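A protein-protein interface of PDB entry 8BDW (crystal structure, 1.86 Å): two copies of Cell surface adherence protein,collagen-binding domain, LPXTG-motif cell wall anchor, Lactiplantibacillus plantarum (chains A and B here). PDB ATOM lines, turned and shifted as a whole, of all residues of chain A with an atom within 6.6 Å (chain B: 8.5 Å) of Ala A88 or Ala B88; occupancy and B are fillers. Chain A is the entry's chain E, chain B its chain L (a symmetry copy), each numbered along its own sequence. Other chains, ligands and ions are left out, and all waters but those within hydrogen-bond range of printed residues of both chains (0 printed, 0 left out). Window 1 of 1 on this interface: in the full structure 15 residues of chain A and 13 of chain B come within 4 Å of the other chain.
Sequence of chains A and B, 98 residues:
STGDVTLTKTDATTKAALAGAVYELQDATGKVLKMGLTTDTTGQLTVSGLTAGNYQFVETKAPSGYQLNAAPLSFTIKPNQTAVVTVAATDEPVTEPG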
ATOM      1  N   THR A   6      25.408   3.453 -29.342  1.00  0.00           N
ATOM      2  CA  THR A   6      26.145   4.210 -30.335  1.00  0.00           C
ATOM      3  C   THR A   6      27.198   5.054 -29.627  1.00  0.00           C
ATOM      4  O   THR A   6      26.912   5.668 -28.598  1.00  0.00           O
ATOM      5  CB  THR A   6      25.158   5.129 -31.120  1.00  0.00           C
ATOM      6  OG1 THR A   6      24.242   4.277 -31.849  1.00  0.00           O
ATOM      7  CG2 THR A   6      25.936   6.098 -32.097  1.00  0.00           C
ATOM      8  N   LEU A   7      28.396   5.137 -30.188  1.00  0.00           N
ATOM      9  CA  LEU A   7      29.400   6.070 -29.702  1.00  0.00           C
ATOM     10  C   LEU A   7      29.625   7.099 -30.795  1.00  0.00           C
ATOM     11  O   LEU A   7      29.712   6.733 -31.964  1.00  0.00           O
ATOM     12  CB  LEU A   7      30.739   5.364 -29.394  1.00  0.00           C
ATOM     13  CG  LEU A   7      32.003   6.156 -29.003  1.00  0.00           C
ATOM     14  CD1 LEU A   7      32.990   5.275 -28.133  1.00  0.00           C
ATOM     15  CD2 LEU A   7      32.817   6.565 -30.261  1.00  0.00           C
ATOM     16  N   THR A   8      29.765   8.375 -30.409  1.00  0.00           N
ATOM     17  CA  THR A   8      30.077   9.446 -31.346  1.00  0.00           C
ATOM     18  C   THR A   8      31.395  10.078 -30.934  1.00  0.00           C
ATOM     19  O   THR A   8      31.576  10.439 -29.770  1.00  0.00           O
ATOM     20  CB  THR A   8      28.965  10.512 -31.378  1.00  0.00           C
ATOM     21  OG1 THR A   8      27.730   9.900 -31.764  1.00  0.00           O
ATOM     22  CG2 THR A   8      29.316  11.668 -32.348  1.00  0.00           C
ATOM     23  N   LYS A   9      32.316  10.185 -31.880  1.00  0.00           N
ATOM     24  CA  LYS A   9      33.676  10.647 -31.642  1.00  0.00           C
ATOM     25  C   LYS A   9      33.886  12.017 -32.285  1.00  0.00           C
ATOM     26  O   LYS A   9      33.617  12.187 -33.482  1.00  0.00           O
ATOM     27  CB  LYS A   9      34.650   9.644 -32.240  1.00  0.00           C
ATOM     28  CG  LYS A   9      36.142   9.964 -31.973  1.00  0.00           C
ATOM     29  CD  LYS A   9      36.438   9.854 -30.474  1.00  0.00           C
ATOM     30  CE  LYS A   9      37.944   9.780 -30.237  1.00  0.00           C
ATOM     31  NZ  LYS A   9      38.532  11.106 -30.402  1.00  0.00           N
ATOM     32  N   THR A  10      34.416  12.970 -31.511  1.00  0.00           N
ATOM     33  CA  THR A  10      34.773  14.289 -32.029  1.00  0.00           C
ATOM     34  C   THR A  10      36.174  14.731 -31.646  1.00  0.00           C
ATOM     35  O   THR A  10      36.858  14.164 -30.770  1.00  0.00           O
ATOM     36  CB  THR A  10      33.810  15.380 -31.507  1.00  0.00           C
ATOM     37  OG1 THR A  10      33.804  15.328 -30.071  1.00  0.00           O
ATOM     38  CG2 THR A  10      32.396  15.110 -32.047  1.00  0.00           C
ATOM     39  N   LEU A  73      35.042   4.403 -21.269  1.00  0.00           N
ATOM     40  CA  LEU A  73      33.767   5.113 -21.347  1.00  0.00           C
ATOM     41  C   LEU A  73      32.666   4.109 -20.990  1.00  0.00           C
ATOM     42  O   LEU A  73      32.301   3.256 -21.809  1.00  0.00           O
ATOM     43  CB  LEU A  73      33.609   5.684 -22.751  1.00  0.00           C
ATOM     44  CG  LEU A  73      32.323   6.355 -23.189  1.00  0.00           C
ATOM     45  CD1 LEU A  73      31.663   7.088 -22.066  1.00  0.00           C
ATOM     46  CD2 LEU A  73      32.700   7.284 -24.343  1.00  0.00           C
ATOM     47  N   THR A  86      23.604   6.154 -25.932  1.00  0.00           N
ATOM     48  CA  THR A  86      24.489   6.944 -26.827  1.00  0.00           C
ATOM     49  C   THR A  86      25.562   7.691 -26.049  1.00  0.00           C
ATOM     50  O   THR A  86      25.226   8.582 -25.265  1.00  0.00           O
ATOM     51  CB  THR A  86      23.759   8.021 -27.667  1.00  0.00           C
ATOM     52  OG1 THR A  86      22.378   8.160 -27.327  1.00  0.00           O
ATOM     53  CG2 THR A  86      23.905   7.764 -29.095  1.00  0.00           C
ATOM     54  N   VAL A  87      26.854   7.400 -26.314  1.00  0.00           N
ATOM     55  CA  VAL A  87      27.953   7.963 -25.543  1.00  0.00           C
ATOM     56  C   VAL A  87      28.789   8.851 -26.447  1.00  0.00           C
ATOM     57  O   VAL A  87      28.892   8.633 -27.660  1.00  0.00           O
ATOM     58  CB  VAL A  87      28.841   6.884 -24.908  1.00  0.00           C
ATOM     59  CG1 VAL A  87      28.032   5.961 -23.926  1.00  0.00           C
ATOM     60  CG2 VAL A  87      29.447   6.033 -25.978  1.00  0.00           C
ATOM     61  N   ALA A  88      29.375   9.874 -25.852  1.00  0.00           N
ATOM     62  CA  ALA A  88      30.137  10.841 -26.613  1.00  0.00           C
ATOM     63  C   ALA A  88      31.576  10.736 -26.161  1.00  0.00           C
ATOM     64  O   ALA A  88      31.848  10.937 -24.975  1.00  0.00           O
ATOM     65  CB  ALA A  88      29.617  12.261 -26.391  1.00  0.00           C
ATOM     66  N   ALA A  89      32.484  10.453 -27.093  1.00  0.00           N
ATOM     67  CA  ALA A  89      33.921  10.449 -26.825  1.00  0.00           C
ATOM     68  C   ALA A  89      34.601  11.599 -27.561  1.00  0.00           C
ATOM     69  O   ALA A  89      34.160  12.013 -28.641  1.00  0.00           O
ATOM     70  CB  ALA A  89      34.541   9.104 -27.252  1.00  0.00           C
ATOM     71  N   THR A  90      35.638  12.173 -26.960  1.00  0.00           N
ATOM     72  CA  THR A  90      36.380  13.247 -27.636  1.00  0.00           C
ATOM     73  C   THR A  90      37.863  12.923 -27.680  1.00  0.00           C
ATOM     74  O   THR A  90      38.375  12.028 -26.958  1.00  0.00           O
ATOM     75  CB  THR A  90      36.165  14.639 -26.973  1.00  0.00           C
ATOM     76  OG1 THR A  90      36.701  14.615 -25.646  1.00  0.00           O
ATOM     77  CG2 THR A  90      34.686  14.976 -26.877  1.00  0.00           C
ATOM     78  N   VAL B   5      25.070  20.166 -38.525  1.00  0.00           N
ATOM     79  CA  VAL B   5      25.249  19.923 -37.095  1.00  0.00           C
ATOM     80  C   VAL B   5      24.231  18.892 -36.645  1.00  0.00           C
ATOM     81  O   VAL B   5      23.094  18.884 -37.120  1.00  0.00           O
ATOM     82  CB  VAL B   5      25.145  21.215 -36.234  1.00  0.00           C
ATOM     83  CG1 VAL B   5      23.809  22.027 -36.455  1.00  0.00           C
ATOM     84  CG2 VAL B   5      25.410  20.934 -34.744  1.00  0.00           C
ATOM     85  N   THR B   6      24.656  17.985 -35.773  1.00  0.00           N
ATOM     86  CA  THR B   6      23.743  17.023 -35.155  1.00  0.00           C
ATOM     87  C   THR B   6      23.838  17.186 -33.652  1.00  0.00           C
ATOM     88  O   THR B   6      24.939  17.298 -33.105  1.00  0.00           O
ATOM     89  CB  THR B   6      24.092  15.581 -35.559  1.00  0.00           C
ATOM     90  OG1 THR B   6      23.890  15.422 -36.976  1.00  0.00           O
ATOM     91  CG2 THR B   6      23.252  14.551 -34.775  1.00  0.00           C
ATOM     92  N   LEU B   7      22.695  17.212 -32.983  1.00  0.00           N
ATOM     93  CA  LEU B   7      22.656  17.202 -31.527  1.00  0.00           C
ATOM     94  C   LEU B   7      22.109  15.847 -31.107  1.00  0.00           C
ATOM     95  O   LEU B   7      21.192  15.346 -31.745  1.00  0.00           O
ATOM     96  CB  LEU B   7      21.742  18.331 -30.994  1.00  0.00           C
ATOM     97  CG  LEU B   7      21.491  18.368 -29.467  1.00  0.00           C
ATOM     98  CD1 LEU B   7      21.252  19.835 -29.031  1.00  0.00           C
ATOM     99  CD2 LEU B   7      20.230  17.515 -29.030  1.00  0.00           C
ATOM    100  N   THR B   8      22.693  15.237 -30.061  1.00  0.00           N
ATOM    101  CA  THR B   8      22.163  13.992 -29.510  1.00  0.00           C
ATOM    102  C   THR B   8      21.766  14.242 -28.059  1.00  0.00           C
ATOM    103  O   THR B   8      22.541  14.816 -27.302  1.00  0.00           O
ATOM    104  CB  THR B   8      23.233  12.853 -29.574  1.00  0.00           C
ATOM    105  OG1 THR B   8      23.659  12.645 -30.927  1.00  0.00           O
ATOM    106  CG2 THR B   8      22.640  11.540 -29.039  1.00  0.00           C
ATOM    107  N   LYS B   9      20.555  13.827 -27.675  1.00  0.00           N
ATOM    108  CA  LYS B   9      19.995  14.105 -26.358  1.00  0.00           C
ATOM    109  C   LYS B   9      19.868  12.805 -25.562  1.00  0.00           C
ATOM    110  O   LYS B   9      19.258  11.846 -26.052  1.00  0.00           O
ATOM    111  CB  LYS B   9      18.614  14.729 -26.478  1.00  0.00           C
ATOM    112  CG  LYS B   9      17.942  15.155 -25.171  1.00  0.00           C
ATOM    113  CD  LYS B   9      18.702  16.354 -24.588  1.00  0.00           C
ATOM    114  CE  LYS B   9      17.911  16.965 -23.480  1.00  0.00           C
ATOM    115  NZ  LYS B   9      17.841  16.088 -22.321  1.00  0.00           N
ATOM    116  N   THR B  10      20.335  12.820 -24.321  1.00  0.00           N
ATOM    117  CA  THR B  10      20.243  11.652 -23.455  1.00  0.00           C
ATOM    118  C   THR B  10      19.727  12.005 -22.066  1.00  0.00           C
ATOM    119  O   THR B  10      19.711  13.165 -21.645  1.00  0.00           O
ATOM    120  CB  THR B  10      21.611  10.942 -23.276  1.00  0.00           C
ATOM    121  OG1 THR B  10      22.558  11.876 -22.735  1.00  0.00           O
ATOM    122  CG2 THR B  10      22.109  10.364 -24.596  1.00  0.00           C
ATOM    123  N   LYS B  15      22.269   7.470 -19.819  1.00  0.00           N
ATOM    124  CA  LYS B  15      22.849   7.697 -21.133  1.00  0.00           C
ATOM    125  C   LYS B  15      21.940   7.202 -22.246  1.00  0.00           C
ATOM    126  O   LYS B  15      22.367   7.070 -23.405  1.00  0.00           O
ATOM    127  CB  LYS B  15      24.253   7.065 -21.240  1.00  0.00           C
ATOM    128  CG  LYS B  15      25.193   7.523 -20.143  1.00  0.00           C
ATOM    129  CD  LYS B  15      26.638   6.976 -20.348  1.00  0.00           C
ATOM    130  CE  LYS B  15      27.515   7.352 -19.117  1.00  0.00           C
ATOM    131  NZ  LYS B  15      28.981   7.236 -19.438  1.00  0.00           N
ATOM    132  N   TYR B  23      14.350  22.228 -29.124  1.00  0.00           N
ATOM    133  CA  TYR B  23      15.436  23.203 -29.115  1.00  0.00           C
ATOM    134  C   TYR B  23      15.159  24.383 -30.053  1.00  0.00           C
ATOM    135  O   TYR B  23      14.544  24.219 -31.115  1.00  0.00           O
ATOM    136  CB  TYR B  23      16.756  22.545 -29.601  1.00  0.00           C
ATOM    137  CG  TYR B  23      17.357  21.712 -28.472  1.00  0.00           C
ATOM    138  CD1 TYR B  23      16.913  20.408 -28.240  1.00  0.00           C
ATOM    139  CD2 TYR B  23      18.268  22.288 -27.588  1.00  0.00           C
ATOM    140  CE1 TYR B  23      17.472  19.636 -27.117  1.00  0.00           C
ATOM    141  CE2 TYR B  23      18.838  21.539 -26.498  1.00  0.00           C
ATOM    142  CZ  TYR B  23      18.403  20.247 -26.282  1.00  0.00           C
ATOM    143  OH  TYR B  23      18.914  19.568 -25.186  1.00  0.00           O
ATOM    144  N   GLY B  43      17.360   9.990 -30.197  1.00  0.00           N
ATOM    145  CA  GLY B  43      17.817  11.150 -29.464  1.00  0.00           C
ATOM    146  C   GLY B  43      18.437  12.241 -30.307  1.00  0.00           C
ATOM    147  O   GLY B  43      18.960  13.203 -29.746  1.00  0.00           O
ATOM    148  N   PHE B  57      22.686  25.912 -29.459  1.00  0.00           N
ATOM    149  CA  PHE B  57      21.383  25.300 -29.218  1.00  0.00           C
ATOM    150  C   PHE B  57      20.916  25.683 -27.823  1.00  0.00           C
ATOM    151  O   PHE B  57      21.704  25.699 -26.876  1.00  0.00           O
ATOM    152  CB  PHE B  57      21.470  23.767 -29.337  1.00  0.00           C
ATOM    153  CG  PHE B  57      21.515  23.257 -30.765  1.00  0.00           C
ATOM    154  CD1 PHE B  57      20.430  23.440 -31.623  1.00  0.00           C
ATOM    155  CD2 PHE B  57      22.615  22.539 -31.226  1.00  0.00           C
ATOM    156  CE1 PHE B  57      20.465  22.943 -32.936  1.00  0.00           C
ATOM    157  CE2 PHE B  57      22.645  22.049 -32.533  1.00  0.00           C
ATOM    158  CZ  PHE B  57      21.591  22.250 -33.373  1.00  0.00           C
ATOM    159  N   LEU B  73      24.305  25.495 -25.707  1.00  0.00           N
ATOM    160  CA  LEU B  73      25.307  24.517 -26.168  1.00  0.00           C
ATOM    161  C   LEU B  73      25.931  25.090 -27.438  1.00  0.00           C
ATOM    162  O   LEU B  73      25.326  25.040 -28.525  1.00  0.00           O
ATOM    163  CB  LEU B  73      24.650  23.165 -26.432  1.00  0.00           C
ATOM    164  CG  LEU B  73      25.453  21.866 -26.348  1.00  0.00           C
ATOM    165  CD1 LEU B  73      26.252  21.859 -25.056  1.00  0.00           C
ATOM    166  CD2 LEU B  73      24.521  20.647 -26.396  1.00  0.00           C
ATOM    167  N   SER B  74      27.113  25.678 -27.293  1.00  0.00           N
ATOM    168  CA  SER B  74      27.764  26.400 -28.387  1.00  0.00           C
ATOM    169  C   SER B  74      28.426  25.482 -29.403  1.00  0.00           C
ATOM    170  O   SER B  74      28.979  24.424 -29.068  1.00  0.00           O
ATOM    171  CB  SER B  74      28.846  27.319 -27.826  1.00  0.00           C
ATOM    172  OG  SER B  74      28.299  28.239 -26.922  1.00  0.00           O
ATOM    173  N   VAL B  85      29.401  18.657 -37.457  1.00  0.00           N
ATOM    174  CA  VAL B  85      29.660  19.031 -36.064  1.00  0.00           C
ATOM    175  C   VAL B  85      28.622  18.327 -35.208  1.00  0.00           C
ATOM    176  O   VAL B  85      27.434  18.317 -35.539  1.00  0.00           O
ATOM    177  CB  VAL B  85      29.585  20.564 -35.888  1.00  0.00           C
ATOM    178  CG1 VAL B  85      29.558  20.919 -34.385  1.00  0.00           C
ATOM    179  CG2 VAL B  85      30.791  21.153 -36.526  1.00  0.00           C
ATOM    180  N   THR B  86      29.015  17.712 -34.089  1.00  0.00           N
ATOM    181  CA  THR B  86      28.025  16.810 -33.483  1.00  0.00           C
ATOM    182  C   THR B  86      28.158  16.855 -31.957  1.00  0.00           C
ATOM    183  O   THR B  86      29.167  16.388 -31.422  1.00  0.00           O
ATOM    184  CB  THR B  86      28.127  15.400 -34.148  1.00  0.00           C
ATOM    185  OG1 THR B  86      27.155  14.456 -33.647  1.00  0.00           O
ATOM    186  CG2 THR B  86      29.537  14.786 -34.096  1.00  0.00           C
ATOM    187  N   VAL B  87      27.143  17.492 -31.282  1.00  0.00           N
ATOM    188  CA  VAL B  87      27.113  17.963 -29.901  1.00  0.00           C
ATOM    189  C   VAL B  87      26.205  17.052 -29.072  1.00  0.00           C
ATOM    190  O   VAL B  87      25.262  16.430 -29.574  1.00  0.00           O
ATOM    191  CB  VAL B  87      26.668  19.442 -29.782  1.00  0.00           C
ATOM    192  CG1 VAL B  87      27.547  20.400 -30.656  1.00  0.00           C
ATOM    193  CG2 VAL B  87      25.212  19.631 -30.151  1.00  0.00           C
ATOM    194  N   ALA B  88      26.532  16.943 -27.789  1.00  0.00           N
ATOM    195  CA  ALA B  88      25.851  16.047 -26.878  1.00  0.00           C
ATOM    196  C   ALA B  88      25.179  16.896 -25.822  1.00  0.00           C
ATOM    197  O   ALA B  88      25.852  17.669 -25.134  1.00  0.00           O
ATOM    198  CB  ALA B  88      26.822  15.072 -26.163  1.00  0.00           C
ATOM    199  N   ALA B  89      23.883  16.683 -25.637  1.00  0.00           N
ATOM    200  CA  ALA B  89      23.100  17.352 -24.610  1.00  0.00           C
ATOM    201  C   ALA B  89      22.519  16.295 -23.690  1.00  0.00           C
ATOM    202  O   ALA B  89      22.151  15.215 -24.156  1.00  0.00           O
ATOM    203  CB  ALA B  89      21.947  18.145 -25.250  1.00  0.00           C
ATOM    204  N   THR B  90      22.428  16.605 -22.393  1.00  0.00           N
ATOM    205  CA  THR B  90      21.890  15.664 -21.404  1.00  0.00           C
ATOM    206  C   THR B  90      20.790  16.327 -20.599  1.00  0.00           C
ATOM    207  O   THR B  90      20.679  17.568 -20.539  1.00  0.00           O
ATOM    208  CB  THR B  90      22.942  15.084 -20.399  1.00  0.00           C
ATOM    209  OG1 THR B  90      23.486  16.132 -19.597  1.00  0.00           O
ATOM    210  CG2 THR B  90      24.089  14.378 -21.134  1.00  0.00           C
ATOM    211  N   ASP B  91      19.933  15.483 -20.011  1.00  0.00           N
ATOM    212  CA  ASP B  91      18.765  15.933 -19.247  1.00  0.00           C
ATOM    213  C   ASP B  91      18.696  15.194 -17.944  1.00  0.00           C
ATOM    214  O   ASP B  91      18.843  13.964 -17.938  1.00  0.00           O
ATOM    215  CB  ASP B  91      17.439  15.670 -19.969  1.00  0.00           C
ATOM    216  CG  ASP B  91      17.285  16.536 -21.189  1.00  0.00           C
ATOM    217  OD1 ASP B  91      16.682  17.603 -21.129  1.00  0.00           O
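The backbone NH of Thr A86 lies within hydrogen-bond range of the backbone carbonyl oxygen of Lys B15.
Thr A8 touches Thr B86, and with the chains exchanged Thr A86 touches Thr B8. Thr A10 touches Thr B86, and with the chains exchanged Thr A86 touches Thr B10. Ala A88 touches its own counterpart, Ala B88. Positions printed for both chains: 6, 7, 8, 9, 10, 73, 86, 87, 88, 89 and 90. Of the 8 pairs that touch across the chains among the printed residues, 5 have their exchanged pair printed and touching as well.
O of Thr A6 is in hydrogen-bond range of N of Val A87. N of Ala A89 is in hydrogen-bond range of O of Thr A8 (2.8 Å). N of Thr B8 is in hydrogen-bond range of O of Val B87 (2.9 Å). The backbone carbonyl oxygen of Thr B8 is in hydrogen-bond range of the backbone NH of Ala B89 (2.8 Å). N of Thr B10 sits at hydrogen-bond distance from O of Ala B89 (3.0 Å). N of Asp B91 sits at hydrogen-bond distance from the backbone carbonyl oxygen (O) of Thr B10, 2.8 Å away.
Ala A88 touches just one residue of chain B: Ala B88 (3.97 Å). No residue of chain B comes within 4 Å of Ala A89. Of the printed residues of chain A, Thr B8 touches Thr A86 (3.8 Å). Of the printed residues of chain A, Thr B10 touches Thr A86. Gly B43 touches none of the printed residues of chain A. Ser B74 touches none of the printed residues of chain A. Of the printed residues of chain A, Thr B86 touches Thr A8 and Thr A10. Ala B88 touches one residue of chain A. The nearest residue of chain B that does not touch Ala A88 is Val B87 (6.5 Å).
Printed residues of chain A that touch a printed residue of chain B: Thr A8, Thr A10, Leu A73, Thr A86, Val A87 and Ala A88. Hydrophobic or aromatic side chains of chain A within 4 Å of the printed part of chain B: Leu A73, Val A87 and Ala A88. Of the 19 printed residues of chain B, 5 touch a printed residue of chain A. Hydrophobic or aromatic side chains of chain B that line the printed part of chain A: Ala B88. Among the printed residues, 8 pairs touch across the chains.
CG2 of Thr A8 touches CG2 of Thr B86, at 3.6 Å. Thr A10 touches Thr B86. Leu A73 touches Lys B15 (CD1 to NZ, 3.8 Å). Thr A86 touches Thr B8 (OG1 to CG2, 3.8 Å). CG2 of Thr B10 touches OG1 of Thr A86 (3.5 Å). Lys B15 touches Val A87. Ala A88 touches Ala B88.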
